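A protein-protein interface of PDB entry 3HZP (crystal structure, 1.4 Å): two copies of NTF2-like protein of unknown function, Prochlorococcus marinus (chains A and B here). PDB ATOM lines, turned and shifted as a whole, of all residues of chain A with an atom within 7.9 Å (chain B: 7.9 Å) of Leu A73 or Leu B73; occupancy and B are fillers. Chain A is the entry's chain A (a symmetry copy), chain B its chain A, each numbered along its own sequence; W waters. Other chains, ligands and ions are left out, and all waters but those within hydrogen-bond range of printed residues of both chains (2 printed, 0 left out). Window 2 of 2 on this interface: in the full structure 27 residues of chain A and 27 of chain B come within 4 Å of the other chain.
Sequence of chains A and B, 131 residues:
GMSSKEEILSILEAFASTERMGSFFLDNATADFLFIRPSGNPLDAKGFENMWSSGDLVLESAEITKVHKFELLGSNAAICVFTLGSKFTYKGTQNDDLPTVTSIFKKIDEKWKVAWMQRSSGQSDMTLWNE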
ATOM      1  N   ILE A   8     -11.163 -18.208  10.381  1.00  0.00           N
ATOM      2  CA  ILE A   8     -12.408 -18.171  11.157  1.00  0.00           C
ATOM      3  C   ILE A   8     -13.134 -19.524  11.064  1.00  0.00           C
ATOM      4  O   ILE A   8     -13.638 -20.029  12.079  1.00  0.00           O
ATOM      5  CB  ILE A   8     -13.229 -16.935  10.751  1.00  0.00           C
ATOM      6  CG1 ILE A   8     -12.508 -15.686  11.344  1.00  0.00           C
ATOM      7  CG2 ILE A   8     -14.708 -17.104  11.171  1.00  0.00           C
ATOM      8  CD1 ILE A   8     -12.800 -14.406  10.612  1.00  0.00           C
ATOM      9  N   LYS A  69     -22.997 -17.376   4.936  1.00  0.00           N
ATOM     10  CA  LYS A  69     -22.498 -16.001   4.796  1.00  0.00           C
ATOM     11  C   LYS A  69     -21.153 -15.927   5.481  1.00  0.00           C
ATOM     12  O   LYS A  69     -20.999 -16.420   6.611  1.00  0.00           O
ATOM     13  CB  LYS A  69     -23.447 -14.988   5.442  1.00  0.00           C
ATOM     14  CG  LYS A  69     -23.024 -13.547   5.305  1.00  0.00           C
ATOM     15  CD  LYS A  69     -24.035 -12.589   5.875  1.00  0.00           C
ATOM     16  CE  LYS A  69     -23.672 -11.164   5.630  1.00  0.00           C
ATOM     17  NZ  LYS A  69     -23.591 -10.836   4.172  1.00  0.00           N
ATOM     18  N   PHE A  70     -20.180 -15.336   4.814  1.00  0.00           N
ATOM     19  CA  PHE A  70     -18.935 -14.984   5.468  1.00  0.00           C
ATOM     20  C   PHE A  70     -18.498 -13.653   4.917  1.00  0.00           C
ATOM     21  O   PHE A  70     -18.416 -13.512   3.695  1.00  0.00           O
ATOM     22  CB  PHE A  70     -17.776 -15.992   5.240  1.00  0.00           C
ATOM     23  CG  PHE A  70     -16.516 -15.467   5.821  1.00  0.00           C
ATOM     24  CD1 PHE A  70     -16.253 -15.620   7.170  1.00  0.00           C
ATOM     25  CD2 PHE A  70     -15.648 -14.704   5.055  1.00  0.00           C
ATOM     26  CE1 PHE A  70     -15.136 -14.971   7.726  1.00  0.00           C
ATOM     27  CE2 PHE A  70     -14.534 -14.097   5.619  1.00  0.00           C
ATOM     28  CZ  PHE A  70     -14.287 -14.236   6.924  1.00  0.00           C
ATOM     29  N   GLU A  71     -18.160 -12.704   5.783  1.00  0.00           N
ATOM     30  CA  GLU A  71     -17.469 -11.524   5.310  1.00  0.00           C
ATOM     31  C   GLU A  71     -16.734 -10.843   6.430  1.00  0.00           C
ATOM     32  O   GLU A  71     -17.162 -10.860   7.580  1.00  0.00           O
ATOM     33  CB  GLU A  71     -18.411 -10.534   4.633  1.00  0.00           C
ATOM     34  CG  GLU A  71     -19.410  -9.924   5.458  1.00  0.00           C
ATOM     35  CD  GLU A  71     -20.281  -8.880   4.684  1.00  0.00           C
ATOM     36  OE1 GLU A  71     -19.769  -8.131   3.834  1.00  0.00           O
ATOM     37  OE2 GLU A  71     -21.454  -8.775   5.014  1.00  0.00           O
ATOM     38  N   LEU A  72     -15.610 -10.245   6.074  1.00  0.00           N
ATOM     39  CA  LEU A  72     -14.921  -9.337   6.979  1.00  0.00           C
ATOM     40  C   LEU A  72     -15.736  -8.077   7.151  1.00  0.00           C
ATOM     41  O   LEU A  72     -16.375  -7.629   6.181  1.00  0.00           O
ATOM     42  CB  LEU A  72     -13.547  -8.970   6.453  1.00  0.00           C
ATOM     43  CG  LEU A  72     -12.516 -10.059   6.465  1.00  0.00           C
ATOM     44  CD1 LEU A  72     -11.214  -9.549   5.815  1.00  0.00           C
ATOM     45  CD2 LEU A  72     -12.188 -10.585   7.901  1.00  0.00           C
ATOM     46  N   LEU A  73     -15.707  -7.523   8.354  1.00  0.00           N
ATOM     47  CA  LEU A  73     -16.362  -6.265   8.699  1.00  0.00           C
ATOM     48  C   LEU A  73     -15.213  -5.378   9.142  1.00  0.00           C
ATOM     49  O   LEU A  73     -14.834  -5.338  10.305  1.00  0.00           O
ATOM     50  CB  LEU A  73     -17.364  -6.512   9.787  1.00  0.00           C
ATOM     51  CG  LEU A  73     -18.513  -7.473   9.439  1.00  0.00           C
ATOM     52  CD1 LEU A  73     -19.387  -7.805  10.631  1.00  0.00           C
ATOM     53  CD2 LEU A  73     -19.343  -6.929   8.244  1.00  0.00           C
ATOM     54  N   GLY A  74     -14.594  -4.745   8.167  1.00  0.00           N
ATOM     55  CA  GLY A  74     -13.295  -4.157   8.352  1.00  0.00           C
ATOM     56  C   GLY A  74     -12.282  -5.238   8.486  1.00  0.00           C
ATOM     57  O   GLY A  74     -12.544  -6.419   8.260  1.00  0.00           O
ATOM     58  N   SER A  75     -11.126  -4.831   8.968  1.00  0.00           N
ATOM     59  CA  SER A  75      -9.980  -5.657   8.978  1.00  0.00           C
ATOM     60  C   SER A  75      -9.972  -6.605  10.188  1.00  0.00           C
ATOM     61  O   SER A  75      -9.361  -7.666  10.144  1.00  0.00           O
ATOM     62  CB  SER A  75      -8.776  -4.714   9.004  1.00  0.00           C
ATOM     63  OG  SER A  75      -9.022  -3.631   8.103  1.00  0.00           O
ATOM     64  N   ASN A  76     -10.682  -6.202  11.231  1.00  0.00           N
ATOM     65  CA  ASN A  76     -10.584  -6.833  12.554  1.00  0.00           C
ATOM     66  C   ASN A  76     -11.866  -7.401  13.113  1.00  0.00           C
ATOM     67  O   ASN A  76     -11.976  -7.648  14.314  1.00  0.00           O
ATOM     68  CB  ASN A  76     -10.021  -5.819  13.566  1.00  0.00           C
ATOM     69  CG  ASN A  76      -8.639  -5.361  13.213  1.00  0.00           C
ATOM     70  OD1 ASN A  76      -7.795  -6.151  12.829  1.00  0.00           O
ATOM     71  ND2 ASN A  76      -8.393  -4.068  13.361  1.00  0.00           N
ATOM     72  N   ALA A  77     -12.869  -7.588  12.248  1.00  0.00           N
ATOM     73  CA  ALA A  77     -14.094  -8.246  12.646  1.00  0.00           C
ATOM     74  C   ALA A  77     -14.654  -9.036  11.467  1.00  0.00           C
ATOM     75  O   ALA A  77     -14.237  -8.841  10.347  1.00  0.00           O
ATOM     76  CB  ALA A  77     -15.132  -7.236  13.193  1.00  0.00           C
ATOM     77  N   ALA A  78     -15.606  -9.895  11.759  1.00  0.00           N
ATOM     78  CA  ALA A  78     -16.228 -10.713  10.724  1.00  0.00           C
ATOM     79  C   ALA A  78     -17.542 -11.253  11.176  1.00  0.00           C
ATOM     80  O   ALA A  78     -17.806 -11.413  12.377  1.00  0.00           O
ATOM     81  CB  ALA A  78     -15.317 -11.876  10.324  1.00  0.00           C
ATOM     82  N   ILE A  79     -18.370 -11.602  10.196  1.00  0.00           N
ATOM     83  CA  ILE A  79     -19.599 -12.322  10.411  1.00  0.00           C
ATOM     84  C   ILE A  79     -19.504 -13.669   9.682  1.00  0.00           C
ATOM     85  O   ILE A  79     -19.083 -13.709   8.536  1.00  0.00           O
ATOM     86  CB  ILE A  79     -20.858 -11.522   9.955  1.00  0.00           C
ATOM     87  CG1 ILE A  79     -22.100 -12.404  10.093  1.00  0.00           C
ATOM     88  CG2 ILE A  79     -20.742 -10.952   8.517  1.00  0.00           C
ATOM     89  CD1 ILE A  79     -23.427 -11.570  10.019  1.00  0.00           C
ATOM     90  N   CYS A  80     -19.977 -14.727  10.344  1.00  0.00           N
ATOM     91  CA  CYS A  80     -20.134 -16.018   9.708  1.00  0.00           C
ATOM     92  C   CYS A  80     -21.462 -16.611  10.129  1.00  0.00           C
ATOM     93  O   CYS A  80     -21.720 -16.800  11.339  1.00  0.00           O
ATOM     94  CB  CYS A  80     -18.957 -16.950  10.026  1.00  0.00           C
ATOM     95  SG  CYS A  80     -19.040 -18.512   9.118  1.00  0.00           S
ATOM     96  N   SER A 103     -22.731 -15.947  13.912  1.00  0.00           N
ATOM     97  CA  SER A 103     -21.552 -15.739  14.770  1.00  0.00           C
ATOM     98  C   SER A 103     -20.821 -14.496  14.321  1.00  0.00           C
ATOM     99  O   SER A 103     -20.787 -14.180  13.116  1.00  0.00           O
ATOM    100  CB  SER A 103     -20.653 -16.964  14.762  1.00  0.00           C
ATOM    101  OG  SER A 103     -20.027 -17.204  13.474  1.00  0.00           O
ATOM    102  N   ILE A 104     -20.225 -13.792  15.271  1.00  0.00           N
ATOM    103  CA  ILE A 104     -19.431 -12.610  15.016  1.00  0.00           C
ATOM    104  C   ILE A 104     -18.065 -12.838  15.667  1.00  0.00           C
ATOM    105  O   ILE A 104     -17.990 -13.422  16.757  1.00  0.00           O
ATOM    106  CB  ILE A 104     -20.068 -11.355  15.594  1.00  0.00           C
ATOM    107  CG1 ILE A 104     -21.503 -11.198  15.096  1.00  0.00           C
ATOM    108  CG2 ILE A 104     -19.194 -10.147  15.375  1.00  0.00           C
ATOM    109  CD1 ILE A 104     -21.582 -11.012  13.645  1.00  0.00           C
ATOM    110  N   PHE A 105     -17.006 -12.433  14.974  1.00  0.00           N
ATOM    111  CA  PHE A 105     -15.621 -12.589  15.389  1.00  0.00           C
ATOM    112  C   PHE A 105     -14.948 -11.219  15.439  1.00  0.00           C
ATOM    113  O   PHE A 105     -15.286 -10.325  14.651  1.00  0.00           O
ATOM    114  CB  PHE A 105     -14.893 -13.474  14.378  1.00  0.00           C
ATOM    115  CG  PHE A 105     -15.289 -14.917  14.474  1.00  0.00           C
ATOM    116  CD1 PHE A 105     -16.436 -15.404  13.920  1.00  0.00           C
ATOM    117  CD2 PHE A 105     -14.443 -15.773  15.154  1.00  0.00           C
ATOM    118  CE1 PHE A 105     -16.748 -16.808  14.143  1.00  0.00           C
ATOM    119  CE2 PHE A 105     -14.722 -17.066  15.321  1.00  0.00           C
ATOM    120  CZ  PHE A 105     -15.858 -17.568  14.836  1.00  0.00           C
ATOM    121  N   LYS A 106     -13.990 -11.076  16.360  1.00  0.00           N
ATOM    122  CA  LYS A 106     -13.156  -9.900  16.446  1.00  0.00           C
ATOM    123  C   LYS A 106     -11.737 -10.304  16.650  1.00  0.00           C
ATOM    124  O   LYS A 106     -11.452 -11.317  17.300  1.00  0.00           O
ATOM    125  CB  LYS A 106     -13.615  -9.011  17.621  1.00  0.00           C
ATOM    126  CG  LYS A 106     -14.972  -8.333  17.382  1.00  0.00           C
ATOM    127  CD  LYS A 106     -15.210  -7.168  18.340  1.00  0.00           C
ATOM    128  CE  LYS A 106     -15.257  -7.703  19.756  1.00  0.00           C
ATOM    129  NZ  LYS A 106     -15.654  -6.602  20.774  1.00  0.00           N
ATOM    130  N   TRP A 112      -7.899 -13.960  16.187  1.00  0.00           N
ATOM    131  CA  TRP A 112      -9.326 -14.055  16.053  1.00  0.00           C
ATOM    132  C   TRP A 112      -9.968 -14.729  17.254  1.00  0.00           C
ATOM    133  O   TRP A 112      -9.515 -15.800  17.690  1.00  0.00           O
ATOM    134  CB  TRP A 112      -9.708 -14.827  14.769  1.00  0.00           C
ATOM    135  CG  TRP A 112      -9.492 -14.072  13.534  1.00  0.00           C
ATOM    136  CD1 TRP A 112      -8.537 -14.308  12.579  1.00  0.00           C
ATOM    137  CD2 TRP A 112     -10.254 -12.967  13.048  1.00  0.00           C
ATOM    138  NE1 TRP A 112      -8.642 -13.403  11.560  1.00  0.00           N
ATOM    139  CE2 TRP A 112      -9.699 -12.569  11.817  1.00  0.00           C
ATOM    140  CE3 TRP A 112     -11.332 -12.265  13.542  1.00  0.00           C
ATOM    141  CZ2 TRP A 112     -10.206 -11.509  11.085  1.00  0.00           C
ATOM    142  CZ3 TRP A 112     -11.841 -11.251  12.812  1.00  0.00           C
ATOM    143  CH2 TRP A 112     -11.280 -10.871  11.604  1.00  0.00           C
ATOM    144  N   ALA A 115     -16.893 -13.420  19.283  1.00  0.00           N
ATOM    145  CA  ALA A 115     -17.428 -12.294  19.992  1.00  0.00           C
ATOM    146  C   ALA A 115     -18.906 -12.428  20.303  1.00  0.00           C
ATOM    147  O   ALA A 115     -19.406 -11.753  21.212  1.00  0.00           O
ATOM    148  CB  ALA A 115     -17.184 -10.996  19.210  1.00  0.00           C
ATOM    149  N   ILE B   8     -27.690   4.329  14.217  1.00  0.00           N
ATOM    150  CA  ILE B   8     -28.140   2.940  14.078  1.00  0.00           C
ATOM    151  C   ILE B   8     -29.407   2.704  14.917  1.00  0.00           C
ATOM    152  O   ILE B   8     -30.353   2.053  14.446  1.00  0.00           O
ATOM    153  CB  ILE B   8     -26.964   1.988  14.350  1.00  0.00           C
ATOM    154  CG1 ILE B   8     -26.001   2.080  13.125  1.00  0.00           C
ATOM    155  CG2 ILE B   8     -27.479   0.566  14.677  1.00  0.00           C
ATOM    156  CD1 ILE B   8     -24.580   1.700  13.435  1.00  0.00           C
ATOM    157  N   LYS B  69     -26.136  -4.699  23.517  1.00  0.00           N
ATOM    158  CA  LYS B  69     -24.780  -4.594  22.961  1.00  0.00           C
ATOM    159  C   LYS B  69     -24.833  -3.639  21.791  1.00  0.00           C
ATOM    160  O   LYS B  69     -25.733  -3.740  20.942  1.00  0.00           O
ATOM    161  CB  LYS B  69     -24.263  -5.952  22.477  1.00  0.00           C
ATOM    162  CG  LYS B  69     -22.858  -5.936  21.929  1.00  0.00           C
ATOM    163  CD  LYS B  69     -22.366  -7.308  21.554  1.00  0.00           C
ATOM    164  CE  LYS B  69     -20.938  -7.304  21.127  1.00  0.00           C
ATOM    165  NZ  LYS B  69     -20.018  -6.835  22.209  1.00  0.00           N
ATOM    166  N   PHE B  70     -23.898  -2.709  21.744  1.00  0.00           N
ATOM    167  CA  PHE B  70     -23.701  -1.911  20.549  1.00  0.00           C
ATOM    168  C   PHE B  70     -22.219  -1.712  20.380  1.00  0.00           C
ATOM    169  O   PHE B  70     -21.565  -1.268  21.326  1.00  0.00           O
ATOM    170  CB  PHE B  70     -24.363  -0.508  20.591  1.00  0.00           C
ATOM    171  CG  PHE B  70     -23.979   0.279  19.393  1.00  0.00           C
ATOM    172  CD1 PHE B  70     -24.652   0.104  18.199  1.00  0.00           C
ATOM    173  CD2 PHE B  70     -22.861   1.099  19.414  1.00  0.00           C
ATOM    174  CE1 PHE B  70     -24.163   0.735  17.040  1.00  0.00           C
ATOM    175  CE2 PHE B  70     -22.413   1.736  18.265  1.00  0.00           C
ATOM    176  CZ  PHE B  70     -23.058   1.558  17.109  1.00  0.00           C
ATOM    177  N   GLU B  71     -21.690  -1.970  19.189  1.00  0.00           N
ATOM    178  CA  GLU B  71     -20.344  -1.526  18.899  1.00  0.00           C
ATOM    179  C   GLU B  71     -20.112  -1.437  17.416  1.00  0.00           C
ATOM    180  O   GLU B  71     -20.667  -2.203  16.634  1.00  0.00           O
ATOM    181  CB  GLU B  71     -19.288  -2.426  19.533  1.00  0.00           C
ATOM    182  CG  GLU B  71     -19.215  -3.774  19.055  1.00  0.00           C
ATOM    183  CD  GLU B  71     -18.060  -4.592  19.722  1.00  0.00           C
ATOM    184  OE1 GLU B  71     -16.964  -4.059  19.970  1.00  0.00           O
ATOM    185  OE2 GLU B  71     -18.254  -5.786  19.905  1.00  0.00           O
ATOM    186  N   LEU B  72     -19.283  -0.479  17.040  1.00  0.00           N
ATOM    187  CA  LEU B  72     -18.763  -0.423  15.682  1.00  0.00           C
ATOM    188  C   LEU B  72     -17.808  -1.571  15.457  1.00  0.00           C
ATOM    189  O   LEU B  72     -17.077  -1.946  16.392  1.00  0.00           O
ATOM    190  CB  LEU B  72     -18.039   0.883  15.420  1.00  0.00           C
ATOM    191  CG  LEU B  72     -18.891   2.114  15.342  1.00  0.00           C
ATOM    192  CD1 LEU B  72     -17.995   3.357  15.168  1.00  0.00           C
ATOM    193  CD2 LEU B  72     -19.928   2.075  14.172  1.00  0.00           C
ATOM    194  N   LEU B  73     -17.815  -2.107  14.246  1.00  0.00           N
ATOM    195  CA  LEU B  73     -16.914  -3.169  13.808  1.00  0.00           C
ATOM    196  C   LEU B  73     -16.159  -2.540  12.652  1.00  0.00           C
ATOM    197  O   LEU B  73     -16.567  -2.602  11.500  1.00  0.00           O
ATOM    198  CB  LEU B  73     -17.722  -4.365  13.399  1.00  0.00           C
ATOM    199  CG  LEU B  73     -18.582  -5.005  14.500  1.00  0.00           C
ATOM    200  CD1 LEU B  73     -19.494  -6.097  13.978  1.00  0.00           C
ATOM    201  CD2 LEU B  73     -17.694  -5.503  15.674  1.00  0.00           C
ATOM    202  N   GLY B  74     -15.102  -1.836  12.998  1.00  0.00           N
ATOM    203  CA  GLY B  74     -14.488  -0.899  12.096  1.00  0.00           C
ATOM    204  C   GLY B  74     -15.388   0.272  11.920  1.00  0.00           C
ATOM    205  O   GLY B  74     -16.385   0.449  12.618  1.00  0.00           O
ATOM    206  N   SER B  75     -15.080   1.032  10.889  1.00  0.00           N
ATOM    207  CA  SER B  75     -15.681   2.293  10.675  1.00  0.00           C
ATOM    208  C   SER B  75     -17.041   2.163   9.971  1.00  0.00           C
ATOM    209  O   SER B  75     -17.899   3.028  10.107  1.00  0.00           O
ATOM    210  CB  SER B  75     -14.693   3.097   9.827  1.00  0.00           C
ATOM    211  OG  SER B  75     -13.372   2.871  10.325  1.00  0.00           O
ATOM    212  N   ASN B  76     -17.210   1.059   9.258  1.00  0.00           N
ATOM    213  CA  ASN B  76     -18.323   0.882   8.315  1.00  0.00           C
ATOM    214  C   ASN B  76     -19.231  -0.296   8.577  1.00  0.00           C
ATOM    215  O   ASN B  76     -19.973  -0.729   7.696  1.00  0.00           O
ATOM    216  CB  ASN B  76     -17.768   0.758   6.884  1.00  0.00           C
ATOM    217  CG  ASN B  76     -17.034   1.987   6.444  1.00  0.00           C
ATOM    218  OD1 ASN B  76     -17.475   3.099   6.677  1.00  0.00           O
ATOM    219  ND2 ASN B  76     -15.905   1.790   5.781  1.00  0.00           N
ATOM    220  N   ALA B  77     -19.159  -0.852   9.792  1.00  0.00           N
ATOM    221  CA  ALA B  77     -20.073  -1.899  10.195  1.00  0.00           C
ATOM    222  C   ALA B  77     -20.355  -1.779  11.691  1.00  0.00           C
ATOM    223  O   ALA B  77     -19.654  -1.084  12.392  1.00  0.00           O
ATOM    224  CB  ALA B  77     -19.528  -3.301   9.833  1.00  0.00           C
ATOM    225  N   ALA B  78     -21.369  -2.488  12.136  1.00  0.00           N
ATOM    226  CA  ALA B  78     -21.745  -2.466  13.544  1.00  0.00           C
ATOM    227  C   ALA B  78     -22.586  -3.644  13.901  1.00  0.00           C
ATOM    228  O   ALA B  78     -23.270  -4.239  13.055  1.00  0.00           O
ATOM    229  CB  ALA B  78     -22.505  -1.182  13.888  1.00  0.00           C
ATOM    230  N   ILE B  79     -22.590  -3.957  15.192  1.00  0.00           N
ATOM    231  CA  ILE B  79     -23.482  -4.928  15.773  1.00  0.00           C
ATOM    232  C   ILE B  79     -24.372  -4.214  16.800  1.00  0.00           C
ATOM    233  O   ILE B  79     -23.870  -3.439  17.600  1.00  0.00           O
ATOM    234  CB  ILE B  79     -22.731  -6.133  16.420  1.00  0.00           C
ATOM    235  CG1 ILE B  79     -23.737  -7.043  17.124  1.00  0.00           C
ATOM    236  CG2 ILE B  79     -21.597  -5.707  17.389  1.00  0.00           C
ATOM    237  CD1 ILE B  79     -23.125  -8.446  17.466  1.00  0.00           C
ATOM    238  N   CYS B  80     -25.660  -4.561  16.799  1.00  0.00           N
ATOM    239  CA  CYS B  80     -26.571  -4.121  17.834  1.00  0.00           C
ATOM    240  C   CYS B  80     -27.448  -5.286  18.240  1.00  0.00           C
ATOM    241  O   CYS B  80     -28.162  -5.871  17.394  1.00  0.00           O
ATOM    242  CB  CYS B  80     -27.394  -2.906  17.383  1.00  0.00           C
ATOM    243  SG  CYS B  80     -28.423  -2.230  18.709  1.00  0.00           S
ATOM    244  N   SER B 103     -28.610  -7.887  15.368  1.00  0.00           N
ATOM    245  CA  SER B 103     -28.636  -7.177  14.079  1.00  0.00           C
ATOM    246  C   SER B 103     -27.239  -6.723  13.730  1.00  0.00           C
ATOM    247  O   SER B 103     -26.442  -6.376  14.623  1.00  0.00           O
ATOM    248  CB  SER B 103     -29.619  -6.018  14.118  1.00  0.00           C
ATOM    249  OG  SER B 103     -29.211  -4.954  15.018  1.00  0.00           O
ATOM    250  N   ILE B 104     -26.933  -6.708  12.442  1.00  0.00           N
ATOM    251  CA  ILE B 104     -25.664  -6.246  11.923  1.00  0.00           C
ATOM    252  C   ILE B 104     -25.971  -5.173  10.875  1.00  0.00           C
ATOM    253  O   ILE B 104     -26.946  -5.307  10.123  1.00  0.00           O
ATOM    254  CB  ILE B 104     -24.862  -7.369  11.282  1.00  0.00           C
ATOM    255  CG1 ILE B 104     -24.691  -8.534  12.255  1.00  0.00           C
ATOM    256  CG2 ILE B 104     -23.574  -6.854  10.691  1.00  0.00           C
ATOM    257  CD1 ILE B 104     -23.922  -8.170  13.448  1.00  0.00           C
ATOM    258  N   PHE B 105     -25.182  -4.104  10.875  1.00  0.00           N
ATOM    259  CA  PHE B 105     -25.322  -2.957   9.993  1.00  0.00           C
ATOM    260  C   PHE B 105     -24.028  -2.759   9.206  1.00  0.00           C
ATOM    261  O   PHE B 105     -22.936  -3.052   9.712  1.00  0.00           O
ATOM    262  CB  PHE B 105     -25.598  -1.712  10.835  1.00  0.00           C
ATOM    263  CG  PHE B 105     -26.984  -1.689  11.406  1.00  0.00           C
ATOM    264  CD1 PHE B 105     -27.332  -2.393  12.521  1.00  0.00           C
ATOM    265  CD2 PHE B 105     -27.932  -0.914  10.765  1.00  0.00           C
ATOM    266  CE1 PHE B 105     -28.726  -2.349  12.938  1.00  0.00           C
ATOM    267  CE2 PHE B 105     -29.199  -0.853  11.177  1.00  0.00           C
ATOM    268  CZ  PHE B 105     -29.588  -1.567  12.234  1.00  0.00           C
ATOM    269  N   LYS B 106     -24.168  -2.250   7.978  1.00  0.00           N
ATOM    270  CA  LYS B 106     -23.043  -1.864   7.158  1.00  0.00           C
ATOM    271  C   LYS B 106     -23.314  -0.545   6.523  1.00  0.00           C
ATOM    272  O   LYS B 106     -24.461  -0.219   6.196  1.00  0.00           O
ATOM    273  CB  LYS B 106     -22.799  -2.925   6.063  1.00  0.00           C
ATOM    274  CG  LYS B 106     -22.261  -4.255   6.609  1.00  0.00           C
ATOM    275  CD  LYS B 106     -21.650  -5.122   5.511  1.00  0.00           C
ATOM    276  CE  LYS B 106     -22.734  -5.490   4.519  1.00  0.00           C
ATOM    277  NZ  LYS B 106     -22.226  -6.502   3.459  1.00  0.00           N
ATOM    278  N   TRP B 112     -25.915   4.096   6.523  1.00  0.00           N
ATOM    279  CA  TRP B 112     -26.124   2.887   7.269  1.00  0.00           C
ATOM    280  C   TRP B 112     -27.318   2.099   6.757  1.00  0.00           C
ATOM    281  O   TRP B 112     -28.406   2.664   6.559  1.00  0.00           O
ATOM    282  CB  TRP B 112     -26.323   3.197   8.772  1.00  0.00           C
ATOM    283  CG  TRP B 112     -25.097   3.591   9.466  1.00  0.00           C
ATOM    284  CD1 TRP B 112     -24.785   4.837   9.946  1.00  0.00           C
ATOM    285  CD2 TRP B 112     -23.996   2.757   9.824  1.00  0.00           C
ATOM    286  NE1 TRP B 112     -23.556   4.828  10.543  1.00  0.00           N
ATOM    287  CE2 TRP B 112     -23.049   3.556  10.492  1.00  0.00           C
ATOM    288  CE3 TRP B 112     -23.710   1.422   9.628  1.00  0.00           C
ATOM    289  CZ2 TRP B 112     -21.852   3.046  10.966  1.00  0.00           C
ATOM    290  CZ3 TRP B 112     -22.556   0.923  10.116  1.00  0.00           C
ATOM    291  CH2 TRP B 112     -21.634   1.725  10.767  1.00  0.00           C
ATOM    292  N   ALA B 115     -27.873  -5.173   7.532  1.00  0.00           N
ATOM    293  CA  ALA B 115     -27.228  -6.212   6.782  1.00  0.00           C
ATOM    294  C   ALA B 115     -27.667  -7.605   7.189  1.00  0.00           C
ATOM    295  O   ALA B 115     -27.508  -8.552   6.409  1.00  0.00           O
ATOM    296  CB  ALA B 115     -25.703  -6.099   6.901  1.00  0.00           C
HETATM  297  O   HOH W   1     -25.442  -8.556   4.445  1.00  0.00           O
HETATM  298  O   HOH W   2     -18.320  -9.237  21.993  1.00  0.00           O
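The side-chain amino group of Lys A106 lies within salt-bridge range of the side-chain carboxylate of Glu B71, at 2.9 Å.
The side-chain amino group (NZ) of Lys B106 is in salt-bridge range of the side-chain carboxylate (OE2) of Glu A71 (2.9 Å).
O of Leu A73 sits close to O of Leu B73 (3.5 Å).
NZ of Lys B69 lies within salt-bridge range of OE2 of Glu B71.
N of Ile B79 sits at hydrogen-bond distance from O of Glu B71, at 3.0 Å.
The backbone carbonyl oxygen of Ile B104 sits at hydrogen-bond distance from the backbone NH of Ala B115, 2.8 Å away.
The side-chain amino group (NZ) of Lys A69 is in salt-bridge range of the side-chain carboxylate (OE2) of Glu A71, at 3.1 Å.
O of Glu A71 sits at hydrogen-bond distance from N of Ile A79, 3.0 Å away.
The backbone NH of Ala A115 is in hydrogen-bond range of the backbone carbonyl oxygen of Ile A104 (2.8 Å).
Among the printed residues, pairs that only touch across the chains: Ile A104 with Ile B104 (3.7 Å), Ala A77 with Leu B73 (3.9 Å), Leu A73 with Ala B77 (3.9 Å), Ile A79 with Ile B104 (3.98 Å) and Ile A104 with Ile B79 (3.98 Å).
Water W1 bridges O of Ala B115 (2.9 Å) and NZ of Lys A69 (2.9 Å).
Water W2 lies within hydrogen-bond range of the backbone carbonyl oxygen (O) of Ala A115 (2.8 Å) and the side-chain amino group (NZ) of Lys B69 (2.9 Å).
Glu A71 touches Lys B106, and with the chains exchanged Lys A106 touches Glu B71.
Leu A73 touches Ala B77, and with the chains exchanged Ala A77 touches Leu B73.
Ile A79 touches Ile B104, and with the chains exchanged Ile A104 touches Ile B79.
Ile B104 touches its own counterpart, Ile A104.
Of the 8 pairs that touch across the chains among the printed residues, 8 have their exchanged pair printed and touching as well.
Of the printed residues of chain B, Leu A73 touches Leu B73 and Ala B77.
Printed residues of chain A within 4 Å of Leu B73: Leu A73 and Ala A77.
No residue of chain B comes within 4 Å of Gly A74.
Ala A77 touches one residue of chain B.
Gly B74 touches none of the printed residues of chain A.
Of chain A, only Leu A73 (3.9 Å) comes within 4 Å of Ala B77.
Of the printed residues of chain B, Lys A106 touches Glu B71 (2.9 Å).
Of the printed residues of chain A, Lys B106 touches Glu A71 (2.9 Å).
Phe A70 touches none of the printed residues of chain B.
Phe B70 touches none of the printed residues of chain A.
The nearest printed residue of chain A that does not touch Leu B73 is Lys A106 (4.01 Å).
Of the 19 printed residues of chain A, 6 touch a printed residue of chain B.
Hydrophobic or aromatic side chains of chain A that line the printed part of chain B: Leu A73, Ala A77, Ile A79 and Ile A104.
Among the printed residues, 8 pairs touch across the chains.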
